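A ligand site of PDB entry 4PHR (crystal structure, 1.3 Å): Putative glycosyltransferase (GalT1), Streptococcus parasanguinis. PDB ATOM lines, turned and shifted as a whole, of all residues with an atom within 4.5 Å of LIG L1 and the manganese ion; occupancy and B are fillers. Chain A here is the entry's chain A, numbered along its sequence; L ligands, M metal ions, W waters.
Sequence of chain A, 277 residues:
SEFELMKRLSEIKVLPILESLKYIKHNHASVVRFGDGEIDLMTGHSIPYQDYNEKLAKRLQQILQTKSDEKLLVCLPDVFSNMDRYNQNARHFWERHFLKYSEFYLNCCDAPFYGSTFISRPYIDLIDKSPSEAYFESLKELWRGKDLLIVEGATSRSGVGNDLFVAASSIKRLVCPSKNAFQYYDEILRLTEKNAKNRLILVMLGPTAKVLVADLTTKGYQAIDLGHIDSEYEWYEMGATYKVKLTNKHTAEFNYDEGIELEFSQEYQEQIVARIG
Water W5 lies within hydrogen-bond range of NH1 of Arg 121 (3.3 Å) and ND1 of His 228 (3.4 Å).
Water W6 lies within hydrogen-bond range of an oxygen (O3) of LIG L1 (2.7 Å) and the backbone carbonyl oxygen (O) of Ser 178 (2.7 Å).
Water W9 lies within hydrogen-bond range of O12 of LIG L1 (2.8 Å), NZ of Lys 210 (2.9 Å) and O of Arg 33 (3.4 Å).
Water W10 lies within hydrogen-bond range of the side-chain hydroxyl (OG1) of Thr 155 (2.7 Å), the side-chain hydroxyl (OG) of Ser 156 (3.0 Å) and an oxygen (O3) of LIG L1 (3.0 Å).
Water W1 lies within hydrogen-bond range of the side-chain amide oxygen (OE1) of Gln 50 (2.7 Å) and an oxygen (O2) of LIG L1 (3.1 Å).
N of Ala 181 lies within hydrogen-bond range of OE1 of Gln 50 (3.5 Å).
The guanidinium group (NH2) of Arg 121 is in salt-bridge range of the side-chain carboxylate (OE1) of Glu 253 (2.6 Å).
The side-chain amino group of Lys 210 lies within salt-bridge range of the side-chain carboxylate of Asp 225, at 2.7 Å.
O of Arg 33 sits close to NZ of Lys 210 (3.2 Å).
A ring nitrogen (NE2) of His 228 lies within hydrogen-bond range of a ring nitrogen (NE2) of His 250 (2.7 Å).
N of His 250 sits at hydrogen-bond distance from O of Thr 155 (2.9 Å).
NH1 of Arg 33 lies within hydrogen-bond range of OG of Ser 120 (3.0 Å).
The side-chain hydroxyl of Ser 156 sits at hydrogen-bond distance from the backbone NH of Gly 153, 3.1 Å away.
The backbone NH (N) of Ala 181 sits at hydrogen-bond distance from an oxygen (O2) of LIG L1 (3.1 Å).
An oxygen (O11) of LIG L1 is in hydrogen-bond range of the backbone NH of His 228 (2.9 Å).
N of Leu 205 is in hydrogen-bond range of O4 of LIG L1.
A ring nitrogen (ND1) of His 228 is in hydrogen-bond range of an oxygen (O9) of LIG L1 (3.2 Å).
O of Ser 178 lies within hydrogen-bond range of N2 of LIG L1, at 3.2 Å.
An oxygen (O8) of LIG L1 lies within salt-bridge range of the side-chain amino group of Lys 210.
NH1 of Arg 121 sits close to O10 of LIG L1, 3.1 Å away.
The side-chain hydroxyl (OG) of Ser 120 sits at hydrogen-bond distance from an oxygen (O11) of LIG L1, at 2.7 Å.
The backbone NH of Gly 206 lies within hydrogen-bond range of an oxygen (O4) of LIG L1.
O12 of LIG L1 is in salt-bridge range of NH1 of Arg 33 (2.8 Å).
The backbone carbonyl oxygen of Pro 177 lies within hydrogen-bond range of a nitrogen (N2) of LIG L1, at 2.9 Å.
The backbone NH (N) of Gly 153 sits close to an oxygen (O1) of LIG L1, 3.2 Å away.
N of Asn 180 is in hydrogen-bond range of O2 of LIG L1 (3.4 Å).
The side-chain hydroxyl (OG) of Ser 156 sits at hydrogen-bond distance from an oxygen (O5) of LIG L1, at 2.9 Å.
Water W7 binds the manganese ion, at 2.2 Å.
The manganese ion is bound by water W2.
The manganese ion is bound by O2 of LG2 L2 (2.2 Å).
The manganese ion is bound by water W4, at 2.2 Å.
O10 of LIG L1 is bound to the manganese ion, at 2.2 Å.
The manganese ion is bound by water W5, at 2.2 Å.
NH1 of Arg 121 touches the manganese ion, at 3.8 Å.
Of the 24 residues printed, 1 comes within 4 Å of the manganese ion.
O2 of LIG L1 sits close to O of Tyr 49, at 3.3 Å.
The backbone carbonyl oxygen of Met 204 sits close to an oxygen (O4) of LIG L1 (3.5 Å).
C of Lys 179 touches O2 of LIG L1 (3.5 Å).
CA of Gly 227 touches O9 of LIG L1, 3.3 Å away.
His 250 touches LIG L1.
The nearest printed residue that does not touch LIG L1 is Asp 225 (4.04 Å).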
ATOM      1  N   ARG A  33      13.731  28.221 -15.745  1.00  0.00           N
ATOM      2  CA  ARG A  33      13.885  29.563 -15.161  1.00  0.00           C
ATOM      3  C   ARG A  33      14.777  30.445 -16.040  1.00  0.00           C
ATOM      4  O   ARG A  33      15.853  30.041 -16.459  1.00  0.00           O
ATOM      5  CB  ARG A  33      14.450  29.485 -13.743  1.00  0.00           C
ATOM      6  CG  ARG A  33      13.672  28.603 -12.741  1.00  0.00           C
ATOM      7  CD  ARG A  33      14.423  28.449 -11.378  1.00  0.00           C
ATOM      8  NE  ARG A  33      15.766  27.987 -11.683  1.00  0.00           N
ATOM      9  CZ  ARG A  33      16.854  28.750 -11.814  1.00  0.00           C
ATOM     10  NH1 ARG A  33      16.842  30.051 -11.503  1.00  0.00           N
ATOM     11  NH2 ARG A  33      17.967  28.175 -12.242  1.00  0.00           N
ATOM     12  N   ASP A  36      19.143  36.593 -15.354  1.00  0.00           N
ATOM     13  CA  ASP A  36      19.836  37.652 -16.071  1.00  0.00           C
ATOM     14  C   ASP A  36      20.794  37.118 -17.123  1.00  0.00           C
ATOM     15  O   ASP A  36      20.903  37.670 -18.209  1.00  0.00           O
ATOM     16  CB  ASP A  36      20.562  38.584 -15.089  1.00  0.00           C
ATOM     17  CG  ASP A  36      21.593  37.872 -14.276  1.00  0.00           C
ATOM     18  OD1 ASP A  36      22.790  38.237 -14.377  1.00  0.00           O
ATOM     19  OD2 ASP A  36      21.210  36.938 -13.537  1.00  0.00           O
ATOM     20  N   TYR A  49      30.381  31.079 -16.861  1.00  0.00           N
ATOM     21  CA  TYR A  49      30.254  29.639 -17.062  1.00  0.00           C
ATOM     22  C   TYR A  49      29.605  29.222 -18.372  1.00  0.00           C
ATOM     23  O   TYR A  49      29.429  28.023 -18.599  1.00  0.00           O
ATOM     24  CB  TYR A  49      29.546  28.969 -15.872  1.00  0.00           C
ATOM     25  CG  TYR A  49      30.195  29.298 -14.539  1.00  0.00           C
ATOM     26  CD1 TYR A  49      31.418  28.733 -14.190  1.00  0.00           C
ATOM     27  CD2 TYR A  49      29.590  30.178 -13.652  1.00  0.00           C
ATOM     28  CE1 TYR A  49      32.018  29.033 -12.987  1.00  0.00           C
ATOM     29  CE2 TYR A  49      30.191  30.478 -12.435  1.00  0.00           C
ATOM     30  CZ  TYR A  49      31.394  29.910 -12.111  1.00  0.00           C
ATOM     31  OH  TYR A  49      31.989  30.201 -10.908  1.00  0.00           O
ATOM     32  N   GLN A  50      29.291  30.167 -19.246  1.00  0.00           N
ATOM     33  CA  GLN A  50      28.832  29.794 -20.592  1.00  0.00           C
ATOM     34  C   GLN A  50      29.126  30.859 -21.642  1.00  0.00           C
ATOM     35  O   GLN A  50      28.565  31.950 -21.624  1.00  0.00           O
ATOM     36  CB  GLN A  50      27.333  29.440 -20.586  1.00  0.00           C
ATOM     37  CG  GLN A  50      26.780  29.042 -21.963  1.00  0.00           C
ATOM     38  CD  GLN A  50      27.425  27.780 -22.515  1.00  0.00           C
ATOM     39  OE1 GLN A  50      27.374  26.711 -21.883  1.00  0.00           O
ATOM     40  NE2 GLN A  50      28.030  27.883 -23.686  1.00  0.00           N
ATOM     41  N   SER A 120      14.894  29.133  -6.950  1.00  0.00           N
ATOM     42  CA  SER A 120      16.234  28.624  -6.628  1.00  0.00           C
ATOM     43  C   SER A 120      16.973  29.580  -5.698  1.00  0.00           C
ATOM     44  O   SER A 120      18.075  29.274  -5.254  1.00  0.00           O
ATOM     45  CB  SER A 120      17.062  28.421  -7.905  1.00  0.00           C
ATOM     46  OG  SER A 120      17.273  29.670  -8.543  1.00  0.00           O
ATOM     47  N   ARG A 121      16.366  30.731  -5.412  1.00  0.00           N
ATOM     48  CA  ARG A 121      17.041  31.834  -4.705  1.00  0.00           C
ATOM     49  C   ARG A 121      16.188  32.370  -3.551  1.00  0.00           C
ATOM     50  O   ARG A 121      15.756  33.522  -3.554  1.00  0.00           O
ATOM     51  CB  ARG A 121      17.357  32.969  -5.702  1.00  0.00           C
ATOM     52  CG  ARG A 121      18.006  32.536  -7.019  1.00  0.00           C
ATOM     53  CD  ARG A 121      19.342  31.844  -6.823  1.00  0.00           C
ATOM     54  NE  ARG A 121      20.231  32.638  -5.993  1.00  0.00           N
ATOM     55  CZ  ARG A 121      21.384  33.146  -6.390  1.00  0.00           C
ATOM     56  NH1 ARG A 121      21.829  32.932  -7.632  1.00  0.00           N
ATOM     57  NH2 ARG A 121      22.106  33.863  -5.548  1.00  0.00           N
ATOM     58  N   GLU A 152      24.078  18.032 -13.070  1.00  0.00           N
ATOM     59  CA  GLU A 152      24.750  19.202 -12.534  1.00  0.00           C
ATOM     60  C   GLU A 152      26.205  19.186 -12.972  1.00  0.00           C
ATOM     61  O   GLU A 152      26.672  18.190 -13.551  1.00  0.00           O
ATOM     62  CB  GLU A 152      24.658  19.220 -11.009  1.00  0.00           C
ATOM     63  CG  GLU A 152      25.369  18.036 -10.374  1.00  0.00           C
ATOM     64  CD  GLU A 152      25.378  18.052  -8.853  1.00  0.00           C
ATOM     65  OE1 GLU A 152      24.758  18.965  -8.249  1.00  0.00           O
ATOM     66  OE2 GLU A 152      26.018  17.151  -8.264  1.00  0.00           O
ATOM     67  N   GLY A 153      26.911  20.269 -12.702  1.00  0.00           N
ATOM     68  CA  GLY A 153      28.306  20.362 -13.071  1.00  0.00           C
ATOM     69  C   GLY A 153      29.224  19.759 -12.032  1.00  0.00           C
ATOM     70  O   GLY A 153      28.812  19.457 -10.901  1.00  0.00           O
ATOM     71  N   THR A 155      31.513  20.985 -10.167  1.00  0.00           N
ATOM     72  CA  THR A 155      31.717  21.742  -8.927  1.00  0.00           C
ATOM     73  C   THR A 155      30.404  22.011  -8.159  1.00  0.00           C
ATOM     74  O   THR A 155      30.440  22.496  -7.024  1.00  0.00           O
ATOM     75  CB  THR A 155      32.449  23.087  -9.182  1.00  0.00           C
ATOM     76  OG1 THR A 155      31.654  23.920 -10.052  1.00  0.00           O
ATOM     77  CG2 THR A 155      33.808  22.851  -9.799  1.00  0.00           C
ATOM     78  N   SER A 156      29.272  21.693  -8.770  1.00  0.00           N
ATOM     79  CA  SER A 156      27.958  22.018  -8.181  1.00  0.00           C
ATOM     80  C   SER A 156      27.736  21.301  -6.852  1.00  0.00           C
ATOM     81  O   SER A 156      27.366  21.918  -5.845  1.00  0.00           O
ATOM     82  CB  SER A 156      26.836  21.650  -9.155  1.00  0.00           C
ATOM     83  OG  SER A 156      26.951  22.367 -10.380  1.00  0.00           O
ATOM     84  N   PRO A 177      30.185  19.278 -17.418  1.00  0.00           N
ATOM     85  CA  PRO A 177      31.201  20.325 -17.232  1.00  0.00           C
ATOM     86  C   PRO A 177      30.682  21.492 -16.408  1.00  0.00           C
ATOM     87  O   PRO A 177      29.511  21.861 -16.525  1.00  0.00           O
ATOM     88  CB  PRO A 177      31.511  20.764 -18.673  1.00  0.00           C
ATOM     89  CG  PRO A 177      31.179  19.565 -19.495  1.00  0.00           C
ATOM     90  CD  PRO A 177      29.947  18.998 -18.847  1.00  0.00           C
ATOM     91  N   SER A 178      31.552  22.054 -15.565  1.00  0.00           N
ATOM     92  CA  SER A 178      31.193  23.193 -14.730  1.00  0.00           C
ATOM     93  C   SER A 178      31.116  24.497 -15.522  1.00  0.00           C
ATOM     94  O   SER A 178      30.591  25.492 -15.036  1.00  0.00           O
ATOM     95  CB  SER A 178      32.200  23.338 -13.584  1.00  0.00           C
ATOM     96  OG  SER A 178      33.506  23.539 -14.086  1.00  0.00           O
ATOM     97  N   LYS A 179      31.643  24.490 -16.732  1.00  0.00           N
ATOM     98  CA  LYS A 179      31.503  25.629 -17.622  1.00  0.00           C
ATOM     99  C   LYS A 179      31.345  25.136 -19.063  1.00  0.00           C
ATOM    100  O   LYS A 179      31.830  24.058 -19.415  1.00  0.00           O
ATOM    101  CB  LYS A 179      32.697  26.581 -17.489  1.00  0.00           C
ATOM    102  CG  LYS A 179      34.013  26.020 -17.982  1.00  0.00           C
ATOM    103  CD  LYS A 179      35.133  27.032 -17.771  1.00  0.00           C
ATOM    104  CE  LYS A 179      36.313  26.747 -18.694  1.00  0.00           C
ATOM    105  NZ  LYS A 179      36.794  25.350 -18.572  1.00  0.00           N
ATOM    106  N   ASN A 180      30.655  25.913 -19.887  1.00  0.00           N
ATOM    107  CA  ASN A 180      30.463  25.559 -21.291  1.00  0.00           C
ATOM    108  C   ASN A 180      29.857  24.182 -21.490  1.00  0.00           C
ATOM    109  O   ASN A 180      30.244  23.443 -22.398  1.00  0.00           O
ATOM    110  CB  ASN A 180      31.765  25.678 -22.077  1.00  0.00           C
ATOM    111  CG  ASN A 180      32.149  27.115 -22.324  1.00  0.00           C
ATOM    112  OD1 ASN A 180      31.317  28.016 -22.208  1.00  0.00           O
ATOM    113  ND2 ASN A 180      33.405  27.339 -22.664  1.00  0.00           N
ATOM    114  N   ALA A 181      28.888  23.839 -20.645  1.00  0.00           N
ATOM    115  CA  ALA A 181      28.266  22.529 -20.765  1.00  0.00           C
ATOM    116  C   ALA A 181      27.508  22.370 -22.088  1.00  0.00           C
ATOM    117  O   ALA A 181      27.308  21.255 -22.549  1.00  0.00           O
ATOM    118  CB  ALA A 181      27.338  22.266 -19.585  1.00  0.00           C
ATOM    119  N   MET A 204      20.875  21.497 -12.501  1.00  0.00           N
ATOM    120  CA  MET A 204      21.609  22.659 -12.007  1.00  0.00           C
ATOM    121  C   MET A 204      22.763  22.877 -12.991  1.00  0.00           C
ATOM    122  O   MET A 204      23.856  22.338 -12.813  1.00  0.00           O
ATOM    123  CB  MET A 204      22.134  22.424 -10.582  1.00  0.00           C
ATOM    124  CG  MET A 204      21.039  22.184  -9.533  1.00  0.00           C
ATOM    125  SD  MET A 204      20.317  20.515  -9.622  1.00  0.00           S
ATOM    126  CE  MET A 204      19.813  20.257  -7.927  1.00  0.00           C
ATOM    127  N   LEU A 205      22.498  23.644 -14.047  1.00  0.00           N
ATOM    128  CA  LEU A 205      23.410  23.643 -15.186  1.00  0.00           C
ATOM    129  C   LEU A 205      23.316  24.906 -16.039  1.00  0.00           C
ATOM    130  O   LEU A 205      23.455  24.854 -17.256  1.00  0.00           O
ATOM    131  CB  LEU A 205      23.206  22.372 -16.043  1.00  0.00           C
ATOM    132  CG  LEU A 205      24.447  21.873 -16.785  1.00  0.00           C
ATOM    133  CD1 LEU A 205      25.466  21.253 -15.821  1.00  0.00           C
ATOM    134  CD2 LEU A 205      24.061  20.868 -17.867  1.00  0.00           C
ATOM    135  N   GLY A 206      23.101  26.045 -15.398  1.00  0.00           N
ATOM    136  CA  GLY A 206      23.118  27.300 -16.114  1.00  0.00           C
ATOM    137  C   GLY A 206      22.179  27.310 -17.298  1.00  0.00           C
ATOM    138  O   GLY A 206      21.082  26.744 -17.227  1.00  0.00           O
ATOM    139  N   LYS A 210      18.127  24.956 -19.174  1.00  0.00           N
ATOM    140  CA  LYS A 210      16.823  25.349 -19.697  1.00  0.00           C
ATOM    141  C   LYS A 210      16.482  24.533 -20.950  1.00  0.00           C
ATOM    142  O   LYS A 210      15.335  24.106 -21.138  1.00  0.00           O
ATOM    143  CB  LYS A 210      16.768  26.841 -19.975  1.00  0.00           C
ATOM    144  CG  LYS A 210      16.877  27.708 -18.703  1.00  0.00           C
ATOM    145  CD  LYS A 210      18.315  27.940 -18.303  1.00  0.00           C
ATOM    146  CE  LYS A 210      18.499  28.889 -17.113  1.00  0.00           C
ATOM    147  NZ  LYS A 210      18.447  28.250 -15.768  1.00  0.00           N
ATOM    148  N   ASP A 225      14.438  22.818 -13.188  1.00  0.00           N
ATOM    149  CA  ASP A 225      15.644  23.645 -13.219  1.00  0.00           C
ATOM    150  C   ASP A 225      15.807  24.318 -11.844  1.00  0.00           C
ATOM    151  O   ASP A 225      15.036  25.217 -11.501  1.00  0.00           O
ATOM    152  CB  ASP A 225      15.410  24.693 -14.310  1.00  0.00           C
ATOM    153  CG  ASP A 225      16.457  25.789 -14.341  1.00  0.00           C
ATOM    154  OD1 ASP A 225      17.471  25.706 -13.619  1.00  0.00           O
ATOM    155  OD2 ASP A 225      16.246  26.736 -15.142  1.00  0.00           O
ATOM    156  N   GLY A 227      19.057  25.373 -10.510  1.00  0.00           N
ATOM    157  CA  GLY A 227      20.143  26.334 -10.472  1.00  0.00           C
ATOM    158  C   GLY A 227      20.978  26.334  -9.212  1.00  0.00           C
ATOM    159  O   GLY A 227      21.556  25.314  -8.843  1.00  0.00           O
ATOM    160  N   HIS A 228      21.040  27.491  -8.545  1.00  0.00           N
ATOM    161  CA  HIS A 228      21.924  27.725  -7.394  1.00  0.00           C
ATOM    162  C   HIS A 228      21.291  27.384  -6.031  1.00  0.00           C
ATOM    163  O   HIS A 228      21.730  27.900  -4.991  1.00  0.00           O
ATOM    164  CB  HIS A 228      22.422  29.170  -7.404  1.00  0.00           C
ATOM    165  CG  HIS A 228      23.619  29.386  -8.279  1.00  0.00           C
ATOM    166  ND1 HIS A 228      23.650  30.343  -9.270  1.00  0.00           N
ATOM    167  CD2 HIS A 228      24.837  28.790  -8.285  1.00  0.00           C
ATOM    168  CE1 HIS A 228      24.847  30.324  -9.858  1.00  0.00           C
ATOM    169  NE2 HIS A 228      25.582  29.391  -9.264  1.00  0.00           N
ATOM    170  N   HIS A 250      31.378  24.883  -5.695  1.00  0.00           N
ATOM    171  CA  HIS A 250      30.962  26.118  -6.356  1.00  0.00           C
ATOM    172  C   HIS A 250      30.074  26.973  -5.444  1.00  0.00           C
ATOM    173  O   HIS A 250      29.221  26.437  -4.738  1.00  0.00           O
ATOM    174  CB  HIS A 250      30.171  25.736  -7.615  1.00  0.00           C
ATOM    175  CG  HIS A 250      29.491  26.892  -8.282  1.00  0.00           C
ATOM    176  ND1 HIS A 250      30.176  27.796  -9.074  1.00  0.00           N
ATOM    177  CD2 HIS A 250      28.203  27.288  -8.287  1.00  0.00           C
ATOM    178  CE1 HIS A 250      29.321  28.693  -9.532  1.00  0.00           C
ATOM    179  NE2 HIS A 250      28.114  28.411  -9.068  1.00  0.00           N
ATOM    180  N   GLU A 253      27.457  33.349  -7.519  1.00  0.00           N
ATOM    181  CA  GLU A 253      27.973  34.723  -7.644  1.00  0.00           C
ATOM    182  C   GLU A 253      29.488  34.847  -7.536  1.00  0.00           C
ATOM    183  O   GLU A 253      30.038  35.941  -7.683  1.00  0.00           O
ATOM    184  CB  GLU A 253      27.245  35.705  -6.731  1.00  0.00           C
ATOM    185  CG  GLU A 253      25.885  36.166  -7.270  1.00  0.00           C
ATOM    186  CD  GLU A 253      24.777  35.165  -7.034  1.00  0.00           C
ATOM    187  OE1 GLU A 253      24.436  34.921  -5.862  1.00  0.00           O
ATOM    188  OE2 GLU A 253      24.237  34.621  -8.020  1.00  0.00           O
HETATM  189  N1  LIG L   1      26.650  25.221 -14.156  1.00  0.00           N
HETATM  190  C1  LIG L   1      27.383  24.145 -14.614  1.00  0.00           C
HETATM  191  N2  LIG L   1      27.846  24.139 -15.910  1.00  0.00           N
HETATM  192  C2  LIG L   1      27.575  25.186 -16.755  1.00  0.00           C
HETATM  193  C3  LIG L   1      26.840  26.274 -16.305  1.00  0.00           C
HETATM  194  C4  LIG L   1      26.510  26.322 -14.953  1.00  0.00           C
HETATM  195  O1  LIG L   1      27.646  23.205 -13.869  1.00  0.00           O
HETATM  196  O2  LIG L   1      27.995  25.121 -17.918  1.00  0.00           O
HETATM  197  C5  LIG L   1      26.097  25.173 -12.800  1.00  0.00           C
HETATM  198  C6  LIG L   1      26.724  25.981 -11.699  1.00  0.00           C
HETATM  199  O3  LIG L   1      27.869  25.330 -11.190  1.00  0.00           O
HETATM  200  C7  LIG L   1      25.589  26.042 -10.706  1.00  0.00           C
HETATM  201  C8  LIG L   1      24.357  26.081 -11.596  1.00  0.00           C
HETATM  202  O4  LIG L   1      24.783  25.685 -12.896  1.00  0.00           O
HETATM  203  O5  LIG L   1      25.554  24.841  -9.946  1.00  0.00           O
HETATM  204  C9  LIG L   1      23.735  27.472 -11.624  1.00  0.00           C
HETATM  205  O6  LIG L   1      22.637  27.449 -12.534  1.00  0.00           O
HETATM  206  P1  LIG L   1      21.765  28.770 -12.847  1.00  0.00           P
HETATM  207  O7  LIG L   1      22.604  29.764 -13.537  1.00  0.00           O
HETATM  208  O8  LIG L   1      20.566  28.299 -13.576  1.00  0.00           O
HETATM  209  O9  LIG L   1      21.419  29.296 -11.358  1.00  0.00           O
HETATM  210  P2  LIG L   1      20.456  30.472 -10.784  1.00  0.00           P
HETATM  211  O10 LIG L   1      21.366  31.572 -10.358  1.00  0.00           O
HETATM  212  O11 LIG L   1      19.779  29.841  -9.626  1.00  0.00           O
HETATM  213  O12 LIG L   1      19.522  30.914 -11.875  1.00  0.00           O
HETATM  214  C1  LG2 L   2      19.879  35.116  -9.645  1.00  0.00           C
HETATM  215  O1  LG2 L   2      19.771  36.012  -8.777  1.00  0.00           O
HETATM  216  O2  LG2 L   2      21.042  34.820 -10.004  1.00  0.00           O
HETATM  217  C2  LG2 L   2      18.659  34.445 -10.220  1.00  0.00           C
HETATM  218 MN    MN M   1      22.136  33.437 -11.337  1.00  0.00          MN
HETATM  219  O   HOH W   1      25.792  26.109 -19.787  1.00  0.00           O
HETATM  220  O   HOH W   2      23.382  32.153 -12.624  1.00  0.00           O
HETATM  221  O   HOH W   3      22.864  31.028 -16.016  1.00  0.00           O
HETATM  222  O   HOH W   4      20.369  33.316 -12.684  1.00  0.00           O
HETATM  223  O   HOH W   5      23.979  33.640 -10.070  1.00  0.00           O
HETATM  224  O   HOH W   6      30.120  26.156 -12.432  1.00  0.00           O
HETATM  225  O   HOH W   7      22.851  35.143 -12.449  1.00  0.00           O
HETATM  226  O   HOH W   8      20.220  25.437 -13.663  1.00  0.00           O
HETATM  227  O   HOH W   9      18.575  30.887 -14.544  1.00  0.00           O
HETATM  228  O   HOH W  10      29.668  22.907 -11.598  1.00  0.00           O
HETATM  229  O   HOH W  11      25.394  29.316 -14.038  1.00  0.00           O
